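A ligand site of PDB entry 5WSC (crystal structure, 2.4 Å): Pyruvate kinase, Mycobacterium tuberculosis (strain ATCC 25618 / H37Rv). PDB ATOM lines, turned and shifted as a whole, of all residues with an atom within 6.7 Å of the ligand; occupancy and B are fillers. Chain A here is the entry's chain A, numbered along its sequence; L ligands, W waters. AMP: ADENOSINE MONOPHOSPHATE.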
ATOM      1  N   ARG A 354       0.032  27.685  -7.567  1.00  0.00           N
ATOM      2  CA  ARG A 354       0.653  26.875  -6.550  1.00  0.00           C
ATOM      3  C   ARG A 354       2.113  26.659  -6.803  1.00  0.00           C
ATOM      4  O   ARG A 354       2.918  26.562  -5.863  1.00  0.00           O
ATOM      5  CB  ARG A 354      -0.063  25.531  -6.418  1.00  0.00           C
ATOM      6  CG  ARG A 354      -1.270  25.628  -5.519  1.00  0.00           C
ATOM      7  CD  ARG A 354      -2.012  24.320  -5.528  1.00  0.00           C
ATOM      8  NE  ARG A 354      -2.661  24.079  -6.809  1.00  0.00           N
ATOM      9  CZ  ARG A 354      -3.479  23.059  -7.024  1.00  0.00           C
ATOM     10  NH1 ARG A 354      -3.746  22.219  -6.041  1.00  0.00           N
ATOM     11  NH2 ARG A 354      -4.032  22.873  -8.193  1.00  0.00           N
ATOM     12  N   ALA A 375       4.400  23.986   4.212  1.00  0.00           N
ATOM     13  CA  ALA A 375       3.298  24.232   3.324  1.00  0.00           C
ATOM     14  C   ALA A 375       2.057  23.433   3.716  1.00  0.00           C
ATOM     15  O   ALA A 375       2.118  22.206   4.000  1.00  0.00           O
ATOM     16  CB  ALA A 375       3.729  23.970   1.907  1.00  0.00           C
ATOM     17  N   PHE A 376       0.931  24.137   3.763  1.00  0.00           N
ATOM     18  CA  PHE A 376      -0.355  23.499   4.004  1.00  0.00           C
ATOM     19  C   PHE A 376      -0.892  22.916   2.708  1.00  0.00           C
ATOM     20  O   PHE A 376      -0.924  23.589   1.704  1.00  0.00           O
ATOM     21  CB  PHE A 376      -1.370  24.501   4.592  1.00  0.00           C
ATOM     22  CG  PHE A 376      -1.250  24.636   6.086  1.00  0.00           C
ATOM     23  CD1 PHE A 376      -0.277  25.426   6.631  1.00  0.00           C
ATOM     24  CD2 PHE A 376      -2.101  23.925   6.925  1.00  0.00           C
ATOM     25  CE1 PHE A 376      -0.122  25.533   7.987  1.00  0.00           C
ATOM     26  CE2 PHE A 376      -1.963  24.027   8.279  1.00  0.00           C
ATOM     27  CZ  PHE A 376      -0.956  24.830   8.815  1.00  0.00           C
ATOM     28  N   THR A 377      -1.326  21.668   2.760  1.00  0.00           N
ATOM     29  CA  THR A 377      -1.840  20.992   1.580  1.00  0.00           C
ATOM     30  C   THR A 377      -2.972  20.013   1.896  1.00  0.00           C
ATOM     31  O   THR A 377      -2.965  19.307   2.891  1.00  0.00           O
ATOM     32  CB  THR A 377      -0.720  20.263   0.837  1.00  0.00           C
ATOM     33  OG1 THR A 377      -1.165  19.934  -0.489  1.00  0.00           O
ATOM     34  CG2 THR A 377      -0.310  19.033   1.615  1.00  0.00           C
ATOM     35  N   GLN A 378      -3.955  20.013   1.031  1.00  0.00           N
ATOM     36  CA  GLN A 378      -5.123  19.218   1.171  1.00  0.00           C
ATOM     37  C   GLN A 378      -5.091  17.994   0.266  1.00  0.00           C
ATOM     38  O   GLN A 378      -5.632  16.961   0.601  1.00  0.00           O
ATOM     39  CB  GLN A 378      -6.282  20.083   0.767  1.00  0.00           C
ATOM     40  CG  GLN A 378      -7.605  19.414   0.790  1.00  0.00           C
ATOM     41  CD  GLN A 378      -8.673  20.418   1.064  1.00  0.00           C
ATOM     42  OE1 GLN A 378      -8.406  21.432   1.735  1.00  0.00           O
ATOM     43  NE2 GLN A 378      -9.897  20.143   0.592  1.00  0.00           N
ATOM     44  N   SER A 379      -4.485  18.141  -0.904  1.00  0.00           N
ATOM     45  CA  SER A 379      -4.284  17.039  -1.839  1.00  0.00           C
ATOM     46  C   SER A 379      -2.799  16.710  -1.985  1.00  0.00           C
ATOM     47  O   SER A 379      -2.459  15.732  -2.635  1.00  0.00           O
ATOM     48  CB  SER A 379      -4.806  17.442  -3.234  1.00  0.00           C
ATOM     49  OG  SER A 379      -3.888  18.314  -3.862  1.00  0.00           O
ATOM     50  N   GLY A 380      -1.920  17.553  -1.448  1.00  0.00           N
ATOM     51  CA  GLY A 380      -0.458  17.358  -1.597  1.00  0.00           C
ATOM     52  C   GLY A 380       0.192  18.215  -2.698  1.00  0.00           C
ATOM     53  O   GLY A 380       1.417  18.306  -2.767  1.00  0.00           O
ATOM     54  N   ASP A 381      -0.623  18.813  -3.566  1.00  0.00           N
ATOM     55  CA  ASP A 381      -0.089  19.434  -4.803  1.00  0.00           C
ATOM     56  C   ASP A 381       0.880  20.546  -4.480  1.00  0.00           C
ATOM     57  O   ASP A 381       2.006  20.552  -4.946  1.00  0.00           O
ATOM     58  CB  ASP A 381      -1.239  19.947  -5.667  1.00  0.00           C
ATOM     59  CG  ASP A 381      -0.749  20.658  -6.908  1.00  0.00           C
ATOM     60  OD1 ASP A 381      -0.399  21.854  -6.775  1.00  0.00           O
ATOM     61  OD2 ASP A 381      -0.652  20.014  -8.002  1.00  0.00           O
ATOM     62  N   THR A 382       0.445  21.464  -3.641  1.00  0.00           N
ATOM     63  CA  THR A 382       1.270  22.621  -3.260  1.00  0.00           C
ATOM     64  C   THR A 382       2.635  22.172  -2.754  1.00  0.00           C
ATOM     65  O   THR A 382       3.654  22.755  -3.102  1.00  0.00           O
ATOM     66  CB  THR A 382       0.569  23.490  -2.167  1.00  0.00           C
ATOM     67  OG1 THR A 382      -0.663  24.024  -2.675  1.00  0.00           O
ATOM     68  CG2 THR A 382       1.423  24.623  -1.766  1.00  0.00           C
ATOM     69  N   VAL A 383       2.677  21.138  -1.938  1.00  0.00           N
ATOM     70  CA  VAL A 383       3.955  20.582  -1.450  1.00  0.00           C
ATOM     71  C   VAL A 383       4.784  19.897  -2.552  1.00  0.00           C
ATOM     72  O   VAL A 383       6.014  19.970  -2.536  1.00  0.00           O
ATOM     73  CB  VAL A 383       3.701  19.574  -0.335  1.00  0.00           C
ATOM     74  CG1 VAL A 383       4.797  18.527  -0.210  1.00  0.00           C
ATOM     75  CG2 VAL A 383       3.488  20.323   0.959  1.00  0.00           C
ATOM     76  N   PHE A 398       1.856  20.346   6.071  1.00  0.00           N
ATOM     77  CA  PHE A 398       0.794  20.289   7.082  1.00  0.00           C
ATOM     78  C   PHE A 398      -0.495  19.969   6.395  1.00  0.00           C
ATOM     79  O   PHE A 398      -0.808  20.533   5.369  1.00  0.00           O
ATOM     80  CB  PHE A 398       0.695  21.606   7.838  1.00  0.00           C
ATOM     81  CG  PHE A 398       1.665  21.719   8.971  1.00  0.00           C
ATOM     82  CD1 PHE A 398       3.012  21.705   8.740  1.00  0.00           C
ATOM     83  CD2 PHE A 398       1.227  21.804  10.259  1.00  0.00           C
ATOM     84  CE1 PHE A 398       3.922  21.758   9.786  1.00  0.00           C
ATOM     85  CE2 PHE A 398       2.125  21.863  11.291  1.00  0.00           C
ATOM     86  CZ  PHE A 398       3.469  21.841  11.058  1.00  0.00           C
ATOM     87  N   THR A 399      -1.257  19.017   6.952  1.00  0.00           N
ATOM     88  CA  THR A 399      -2.500  18.622   6.358  1.00  0.00           C
ATOM     89  C   THR A 399      -3.467  18.182   7.431  1.00  0.00           C
ATOM     90  O   THR A 399      -3.035  17.880   8.562  1.00  0.00           O
ATOM     91  CB  THR A 399      -2.265  17.498   5.316  1.00  0.00           C
ATOM     92  OG1 THR A 399      -3.431  17.312   4.504  1.00  0.00           O
ATOM     93  CG2 THR A 399      -1.921  16.211   5.998  1.00  0.00           C
ATOM     94  N   ALA A 400      -4.763  18.209   7.116  1.00  0.00           N
ATOM     95  CA  ALA A 400      -5.784  17.600   7.991  1.00  0.00           C
ATOM     96  C   ALA A 400      -6.232  16.238   7.492  1.00  0.00           C
ATOM     97  O   ALA A 400      -7.028  15.561   8.177  1.00  0.00           O
ATOM     98  CB  ALA A 400      -7.002  18.493   8.147  1.00  0.00           C
ATOM     99  N   TRP A 401      -5.734  15.808   6.341  1.00  0.00           N
ATOM    100  CA  TRP A 401      -6.107  14.508   5.780  1.00  0.00           C
ATOM    101  C   TRP A 401      -4.936  13.531   5.916  1.00  0.00           C
ATOM    102  O   TRP A 401      -3.905  13.654   5.223  1.00  0.00           O
ATOM    103  CB  TRP A 401      -6.585  14.672   4.335  1.00  0.00           C
ATOM    104  CG  TRP A 401      -7.798  15.579   4.299  1.00  0.00           C
ATOM    105  CD1 TRP A 401      -9.114  15.200   4.298  1.00  0.00           C
ATOM    106  CD2 TRP A 401      -7.797  17.018   4.365  1.00  0.00           C
ATOM    107  NE1 TRP A 401      -9.924  16.299   4.317  1.00  0.00           N
ATOM    108  CE2 TRP A 401      -9.138  17.427   4.359  1.00  0.00           C
ATOM    109  CE3 TRP A 401      -6.787  17.993   4.440  1.00  0.00           C
ATOM    110  CZ2 TRP A 401      -9.508  18.780   4.432  1.00  0.00           C
ATOM    111  CZ3 TRP A 401      -7.160  19.334   4.468  1.00  0.00           C
ATOM    112  CH2 TRP A 401      -8.493  19.720   4.458  1.00  0.00           C
ATOM    113  N   VAL A 419      -2.842  17.942  11.425  1.00  0.00           N
ATOM    114  CA  VAL A 419      -3.433  18.839  12.411  1.00  0.00           C
ATOM    115  C   VAL A 419      -4.932  18.888  12.151  1.00  0.00           C
ATOM    116  O   VAL A 419      -5.394  18.430  11.083  1.00  0.00           O
ATOM    117  CB  VAL A 419      -2.847  20.265  12.287  1.00  0.00           C
ATOM    118  CG1 VAL A 419      -1.346  20.267  12.555  1.00  0.00           C
ATOM    119  CG2 VAL A 419      -3.100  20.822  10.863  1.00  0.00           C
ATOM    120  N   PRO A 420      -5.701  19.465  13.098  1.00  0.00           N
ATOM    121  CA  PRO A 420      -7.123  19.602  12.925  1.00  0.00           C
ATOM    122  C   PRO A 420      -7.482  20.361  11.681  1.00  0.00           C
ATOM    123  O   PRO A 420      -6.662  21.130  11.143  1.00  0.00           O
ATOM    124  CB  PRO A 420      -7.529  20.369  14.167  1.00  0.00           C
ATOM    125  CG  PRO A 420      -6.606  19.851  15.216  1.00  0.00           C
ATOM    126  CD  PRO A 420      -5.302  19.777  14.482  1.00  0.00           C
ATOM    127  N   LYS A 421      -8.668  20.109  11.188  1.00  0.00           N
ATOM    128  CA  LYS A 421      -9.231  20.881  10.106  1.00  0.00           C
ATOM    129  C   LYS A 421      -9.528  22.310  10.609  1.00  0.00           C
ATOM    130  O   LYS A 421     -10.350  22.468  11.490  1.00  0.00           O
ATOM    131  CB  LYS A 421     -10.507  20.194   9.584  1.00  0.00           C
ATOM    132  CG  LYS A 421     -11.150  20.892   8.411  1.00  0.00           C
ATOM    133  CD  LYS A 421     -12.393  20.178   7.975  1.00  0.00           C
ATOM    134  CE  LYS A 421     -12.434  20.142   6.447  1.00  0.00           C
ATOM    135  NZ  LYS A 421     -13.757  20.479   5.841  1.00  0.00           N
ATOM    136  N   MET A 422      -8.824  23.317  10.083  1.00  0.00           N
ATOM    137  CA  MET A 422      -8.877  24.664  10.662  1.00  0.00           C
ATOM    138  C   MET A 422      -9.745  25.581   9.833  1.00  0.00           C
ATOM    139  O   MET A 422      -9.934  25.391   8.633  1.00  0.00           O
ATOM    140  CB  MET A 422      -7.485  25.331  10.760  1.00  0.00           C
ATOM    141  CG  MET A 422      -6.413  24.481  11.396  1.00  0.00           C
ATOM    142  SD  MET A 422      -6.836  23.987  13.067  1.00  0.00           S
ATOM    143  CE  MET A 422      -7.056  25.537  13.921  1.00  0.00           C
ATOM    144  N   GLN A 423     -10.235  26.627  10.486  1.00  0.00           N
ATOM    145  CA  GLN A 423     -11.271  27.432   9.911  1.00  0.00           C
ATOM    146  C   GLN A 423     -10.754  28.802   9.584  1.00  0.00           C
ATOM    147  O   GLN A 423     -11.536  29.690   9.262  1.00  0.00           O
ATOM    148  CB  GLN A 423     -12.464  27.441  10.854  1.00  0.00           C
ATOM    149  CG  GLN A 423     -13.219  26.112  10.805  1.00  0.00           C
ATOM    150  CD  GLN A 423     -13.390  25.391  12.177  1.00  0.00           C
ATOM    151  OE1 GLN A 423     -12.403  25.040  12.863  1.00  0.00           O
ATOM    152  NE2 GLN A 423     -14.647  25.105  12.541  1.00  0.00           N
ATOM    153  N   SER A 424      -9.421  28.970   9.653  1.00  0.00           N
ATOM    154  CA  SER A 424      -8.781  30.234   9.285  1.00  0.00           C
ATOM    155  C   SER A 424      -7.254  30.057   9.160  1.00  0.00           C
ATOM    156  O   SER A 424      -6.671  29.093   9.709  1.00  0.00           O
ATOM    157  CB  SER A 424      -9.062  31.308  10.330  1.00  0.00           C
ATOM    158  OG  SER A 424      -8.227  31.144  11.464  1.00  0.00           O
ATOM    159  N   THR A 425      -6.606  30.981   8.436  1.00  0.00           N
ATOM    160  CA  THR A 425      -5.144  30.919   8.265  1.00  0.00           C
ATOM    161  C   THR A 425      -4.361  31.230   9.564  1.00  0.00           C
ATOM    162  O   THR A 425      -3.276  30.665   9.808  1.00  0.00           O
ATOM    163  CB  THR A 425      -4.662  31.842   7.101  1.00  0.00           C
ATOM    164  OG1 THR A 425      -5.243  33.128   7.208  1.00  0.00           O
ATOM    165  CG2 THR A 425      -5.066  31.271   5.740  1.00  0.00           C
ATOM    166  N   MET A 428      -4.183  28.057  11.122  1.00  0.00           N
ATOM    167  CA  MET A 428      -3.152  27.232  10.477  1.00  0.00           C
ATOM    168  C   MET A 428      -1.786  27.506  11.107  1.00  0.00           C
ATOM    169  O   MET A 428      -1.022  26.571  11.477  1.00  0.00           O
ATOM    170  CB  MET A 428      -3.156  27.470   8.961  1.00  0.00           C
ATOM    171  CG  MET A 428      -4.459  26.978   8.303  1.00  0.00           C
ATOM    172  SD  MET A 428      -4.554  26.992   6.497  1.00  0.00           S
ATOM    173  CE  MET A 428      -6.267  27.268   6.189  1.00  0.00           C
ATOM    174  N   GLN A 431      -1.224  26.346  14.716  1.00  0.00           N
ATOM    175  CA  GLN A 431      -0.991  24.893  14.670  1.00  0.00           C
ATOM    176  C   GLN A 431       0.434  24.581  14.305  1.00  0.00           C
ATOM    177  O   GLN A 431       1.002  23.609  14.808  1.00  0.00           O
ATOM    178  CB  GLN A 431      -1.925  24.187  13.675  1.00  0.00           C
ATOM    179  CG  GLN A 431      -3.315  23.903  14.193  1.00  0.00           C
ATOM    180  CD  GLN A 431      -3.321  23.200  15.533  1.00  0.00           C
ATOM    181  OE1 GLN A 431      -2.574  22.216  15.742  1.00  0.00           O
ATOM    182  NE2 GLN A 431      -4.126  23.709  16.450  1.00  0.00           N
ATOM    183  N   VAL A 451       3.417  28.585   3.856  1.00  0.00           N
ATOM    184  CA  VAL A 451       2.493  28.731   2.746  1.00  0.00           C
ATOM    185  C   VAL A 451       1.126  28.233   3.174  1.00  0.00           C
ATOM    186  O   VAL A 451       1.011  27.167   3.747  1.00  0.00           O
ATOM    187  CB  VAL A 451       2.944  27.879   1.538  1.00  0.00           C
ATOM    188  CG1 VAL A 451       1.945  27.972   0.384  1.00  0.00           C
ATOM    189  CG2 VAL A 451       4.315  28.295   1.083  1.00  0.00           C
ATOM    190  N   ALA A 452       0.095  28.981   2.885  1.00  0.00           N
ATOM    191  CA  ALA A 452      -1.233  28.516   3.186  1.00  0.00           C
ATOM    192  C   ALA A 452      -2.185  29.164   2.234  1.00  0.00           C
ATOM    193  O   ALA A 452      -1.733  29.822   1.275  1.00  0.00           O
ATOM    194  CB  ALA A 452      -1.598  28.841   4.606  1.00  0.00           C
ATOM    195  N   GLY A 453      -3.485  28.979   2.474  1.00  0.00           N
ATOM    196  CA  GLY A 453      -4.488  29.401   1.502  1.00  0.00           C
ATOM    197  C   GLY A 453      -5.855  29.589   2.134  1.00  0.00           C
ATOM    198  O   GLY A 453      -6.217  28.911   3.105  1.00  0.00           O
ATOM    199  N   ALA A 454      -6.610  30.525   1.578  1.00  0.00           N
ATOM    200  CA  ALA A 454      -8.017  30.741   1.966  1.00  0.00           C
ATOM    201  C   ALA A 454      -8.783  30.912   0.682  1.00  0.00           C
ATOM    202  O   ALA A 454      -8.215  31.399  -0.300  1.00  0.00           O
ATOM    203  CB  ALA A 454      -8.174  31.966   2.853  1.00  0.00           C
ATOM    204  N   PRO A 455     -10.054  30.507   0.630  1.00  0.00           N
ATOM    205  CA  PRO A 455     -10.768  29.885   1.728  1.00  0.00           C
ATOM    206  C   PRO A 455     -10.183  28.562   2.248  1.00  0.00           C
ATOM    207  O   PRO A 455      -9.727  27.735   1.461  1.00  0.00           O
ATOM    208  CB  PRO A 455     -12.154  29.623   1.120  1.00  0.00           C
ATOM    209  CG  PRO A 455     -11.953  29.584  -0.349  1.00  0.00           C
ATOM    210  CD  PRO A 455     -10.625  30.182  -0.671  1.00  0.00           C
ATOM    211  N   PRO A 456     -10.296  28.326   3.559  1.00  0.00           N
ATOM    212  CA  PRO A 456      -9.812  27.092   4.177  1.00  0.00           C
ATOM    213  C   PRO A 456     -10.515  25.836   3.663  1.00  0.00           C
ATOM    214  O   PRO A 456     -11.690  25.882   3.269  1.00  0.00           O
ATOM    215  CB  PRO A 456     -10.150  27.259   5.653  1.00  0.00           C
ATOM    216  CG  PRO A 456     -10.573  28.671   5.839  1.00  0.00           C
ATOM    217  CD  PRO A 456     -11.075  29.142   4.499  1.00  0.00           C
ATOM    218  N   GLY A 457      -9.802  24.725   3.704  1.00  0.00           N
ATOM    219  CA  GLY A 457     -10.356  23.493   3.201  1.00  0.00           C
ATOM    220  C   GLY A 457     -10.688  23.510   1.718  1.00  0.00           C
ATOM    221  O   GLY A 457     -11.533  22.785   1.290  1.00  0.00           O
ATOM    222  N   THR A 458      -9.988  24.284   0.910  1.00  0.00           N
ATOM    223  CA  THR A 458     -10.245  24.305  -0.550  1.00  0.00           C
ATOM    224  C   THR A 458      -8.977  23.888  -1.329  1.00  0.00           C
ATOM    225  O   THR A 458      -7.921  24.491  -1.173  1.00  0.00           O
ATOM    226  CB  THR A 458     -10.773  25.700  -0.989  1.00  0.00           C
ATOM    227  OG1 THR A 458     -12.000  25.981  -0.292  1.00  0.00           O
ATOM    228  CG2 THR A 458     -11.085  25.770  -2.504  1.00  0.00           C
ATOM    229  N   VAL A 459      -9.055  22.800  -2.094  1.00  0.00           N
ATOM    230  CA  VAL A 459      -7.882  22.385  -2.889  1.00  0.00           C
ATOM    231  C   VAL A 459      -7.532  23.526  -3.859  1.00  0.00           C
ATOM    232  O   VAL A 459      -8.405  24.118  -4.488  1.00  0.00           O
ATOM    233  CB  VAL A 459      -8.139  21.051  -3.632  1.00  0.00           C
ATOM    234  CG1 VAL A 459      -7.096  20.750  -4.694  1.00  0.00           C
ATOM    235  CG2 VAL A 459      -8.209  19.930  -2.624  1.00  0.00           C
ATOM    236  N   GLY A 460      -6.256  23.886  -3.915  1.00  0.00           N
ATOM    237  CA  GLY A 460      -5.781  24.962  -4.811  1.00  0.00           C
ATOM    238  C   GLY A 460      -6.109  26.376  -4.400  1.00  0.00           C
ATOM    239  O   GLY A 460      -6.081  27.283  -5.223  1.00  0.00           O
ATOM    240  N   SER A 461      -6.437  26.590  -3.131  1.00  0.00           N
ATOM    241  CA  SER A 461      -6.710  27.954  -2.665  1.00  0.00           C
ATOM    242  C   SER A 461      -5.423  28.598  -2.214  1.00  0.00           C
ATOM    243  O   SER A 461      -5.393  29.780  -1.863  1.00  0.00           O
ATOM    244  CB  SER A 461      -7.756  27.984  -1.517  1.00  0.00           C
ATOM    245  OG  SER A 461      -7.254  27.334  -0.357  1.00  0.00           O
ATOM    246  N   THR A 462      -4.345  27.823  -2.198  1.00  0.00           N
ATOM    247  CA  THR A 462      -3.037  28.321  -1.804  1.00  0.00           C
ATOM    248  C   THR A 462      -2.811  29.760  -2.285  1.00  0.00           C
ATOM    249  O   THR A 462      -2.825  30.008  -3.498  1.00  0.00           O
ATOM    250  CB  THR A 462      -1.957  27.430  -2.354  1.00  0.00           C
ATOM    251  OG1 THR A 462      -2.143  26.092  -1.860  1.00  0.00           O
ATOM    252  CG2 THR A 462      -0.582  27.952  -1.921  1.00  0.00           C
ATOM    253  N   ASN A 463      -2.612  30.694  -1.360  1.00  0.00           N
ATOM    254  CA  ASN A 463      -2.441  32.090  -1.746  1.00  0.00           C
ATOM    255  C   ASN A 463      -1.735  32.993  -0.733  1.00  0.00           C
ATOM    256  O   ASN A 463      -1.732  34.206  -0.884  1.00  0.00           O
ATOM    257  CB  ASN A 463      -3.773  32.695  -2.180  1.00  0.00           C
ATOM    258  CG  ASN A 463      -4.751  32.842  -1.035  1.00  0.00           C
ATOM    259  OD1 ASN A 463      -4.452  32.475   0.107  1.00  0.00           O
ATOM    260  ND2 ASN A 463      -5.893  33.433  -1.317  1.00  0.00           N
HETATM  261  P   AMP L   1      -3.689  21.928  -2.219  1.00  0.00           P
HETATM  262  O1P AMP L   1      -2.208  21.680  -2.007  1.00  0.00           O
HETATM  263  O2P AMP L   1      -3.899  23.065  -3.178  1.00  0.00           O
HETATM  264  O3P AMP L   1      -4.461  20.699  -2.649  1.00  0.00           O
HETATM  265  O5' AMP L   1      -4.253  22.377  -0.784  1.00  0.00           O
HETATM  266  C5' AMP L   1      -3.760  23.556  -0.129  1.00  0.00           C
HETATM  267  C4' AMP L   1      -4.899  24.168   0.701  1.00  0.00           C
HETATM  268  O4' AMP L   1      -5.523  23.147   1.498  1.00  0.00           O
HETATM  269  C3' AMP L   1      -4.452  25.231   1.699  1.00  0.00           C
HETATM  270  O3' AMP L   1      -4.398  26.546   1.153  1.00  0.00           O
HETATM  271  C2' AMP L   1      -5.512  25.163   2.772  1.00  0.00           C
HETATM  272  O2' AMP L   1      -6.568  26.081   2.472  1.00  0.00           O
HETATM  273  C1' AMP L   1      -6.033  23.729   2.715  1.00  0.00           C
HETATM  274  N9  AMP L   1      -5.543  23.142   3.956  1.00  0.00           N
HETATM  275  C8  AMP L   1      -4.341  22.601   4.266  1.00  0.00           C
HETATM  276  N7  AMP L   1      -4.317  22.215   5.573  1.00  0.00           N
HETATM  277  C5  AMP L   1      -5.488  22.571   6.063  1.00  0.00           C
HETATM  278  C6  AMP L   1      -6.104  22.457   7.352  1.00  0.00           C
HETATM  279  N6  AMP L   1      -5.387  21.912   8.327  1.00  0.00           N
HETATM  280  N1  AMP L   1      -7.341  22.907   7.514  1.00  0.00           N
HETATM  281  C2  AMP L   1      -8.024  23.459   6.500  1.00  0.00           C
HETATM  282  N3  AMP L   1      -7.512  23.583   5.275  1.00  0.00           N
HETATM  283  C4  AMP L   1      -6.276  23.162   5.017  1.00  0.00           C
HETATM  284  O   HOH W   1      -1.098  26.130   0.931  1.00  0.00           O
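N of Phe 376 sits at hydrogen-bond distance from O of Val 451, 3.0 Å away.
The side-chain hydroxyl (OG1) of Thr 377 sits at hydrogen-bond distance from the backbone NH (N) of Gly 380 (2.7 Å).
N of Trp 401 sits at hydrogen-bond distance from OG1 of Thr 399 (3.3 Å).
OG of Ser 379 is in hydrogen-bond range of N of Asp 381, 3.3 Å away.
The side-chain hydroxyl of Thr 382 sits at hydrogen-bond distance from the side-chain hydroxyl of Thr 462, at 2.7 Å.
The backbone carbonyl oxygen (O) of Ala 452 sits at hydrogen-bond distance from the backbone NH (N) of Asn 463, 2.9 Å away.
The backbone NH (N) of Val 419 lies within hydrogen-bond range of the backbone carbonyl oxygen (O) of Thr 399.
The side-chain amide oxygen of Asn 463 sits close to the backbone carbonyl oxygen of Ser 461 (3.5 Å).
Water W1 lies within hydrogen-bond range of the backbone carbonyl oxygen of Phe 376 (2.7 Å), the side-chain hydroxyl of Thr 462 (3.0 Å) and an oxygen (O3') of the ligand (3.3 Å).
OG of Ser 379 sits at hydrogen-bond distance from O3P of the ligand (2.7 Å).
A nitrogen (N3) of the ligand sits at hydrogen-bond distance from the backbone NH (N) of Gly 457, 3.0 Å away.
The backbone NH (N) of Thr 382 is in hydrogen-bond range of an oxygen (O1P) of the ligand (3.1 Å).
O2P of the ligand lies within hydrogen-bond range of N of Gly 460, at 2.6 Å.
The side-chain hydroxyl of Thr 377 is in hydrogen-bond range of an oxygen (O1P) of the ligand, at 2.5 Å.
O of Gly 453 sits at hydrogen-bond distance from O2' of the ligand, at 2.9 Å.
An oxygen (O2P) of the ligand lies within salt-bridge range of the guanidinium group (NH1) of Arg 354, 3.0 Å away.
The backbone NH (N) of Met 422 sits at hydrogen-bond distance from a nitrogen (N1) of the ligand, at 3.0 Å.
O4' of the ligand lies close to OE1 of Gln 378 (3.4 Å).
The backbone NH (N) of Ser 379 lies within hydrogen-bond range of an oxygen (O3P) of the ligand, 3.1 Å away.
An oxygen (O1P) of the ligand lies within hydrogen-bond range of the side-chain hydroxyl of Thr 382, at 2.9 Å.
The backbone carbonyl oxygen (O) of Pro 420 sits at hydrogen-bond distance from a nitrogen (N6) of the ligand, at 3.2 Å.
The backbone NH of Gly 453 sits close to an oxygen (O3') of the ligand (2.9 Å).
N of Gln 378 is in hydrogen-bond range of O5' of the ligand.
An oxygen (O2') of the ligand is in hydrogen-bond range of the side-chain hydroxyl (OG) of Ser 461 (3.2 Å).
Phe 376 touches the ligand.
Asp 381 touches the ligand (N to O1P, 3.6 Å).
Phe 398 touches the ligand.
Ala 400 touches the ligand.
CZ3 of Trp 401 touches C4 of the ligand, 3.97 Å away.
Val 419 touches the ligand (CG2 to N6, 3.6 Å).
CA of Lys 421 touches N1 of the ligand, at 3.8 Å.
CE of Met 428 touches O2' of the ligand, at 3.9 Å.
C of Ala 452 touches O3' of the ligand (3.6 Å).
O of Pro 455 touches O2' of the ligand (3.7 Å).
Pro 456 touches the ligand.
O of Thr 458 touches C4' of the ligand (3.6 Å).
Val 459 touches the ligand (CG1 to O3P, 3.3 Å).
Thr 462 touches the ligand.
Hydrophobic or aromatic side chains that line the ligand: Phe 376, Ala 400, Trp 401, Val 419, Met 428 and Val 459.
Of the 36 residues printed, 25 come within 4 Å of the ligand.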
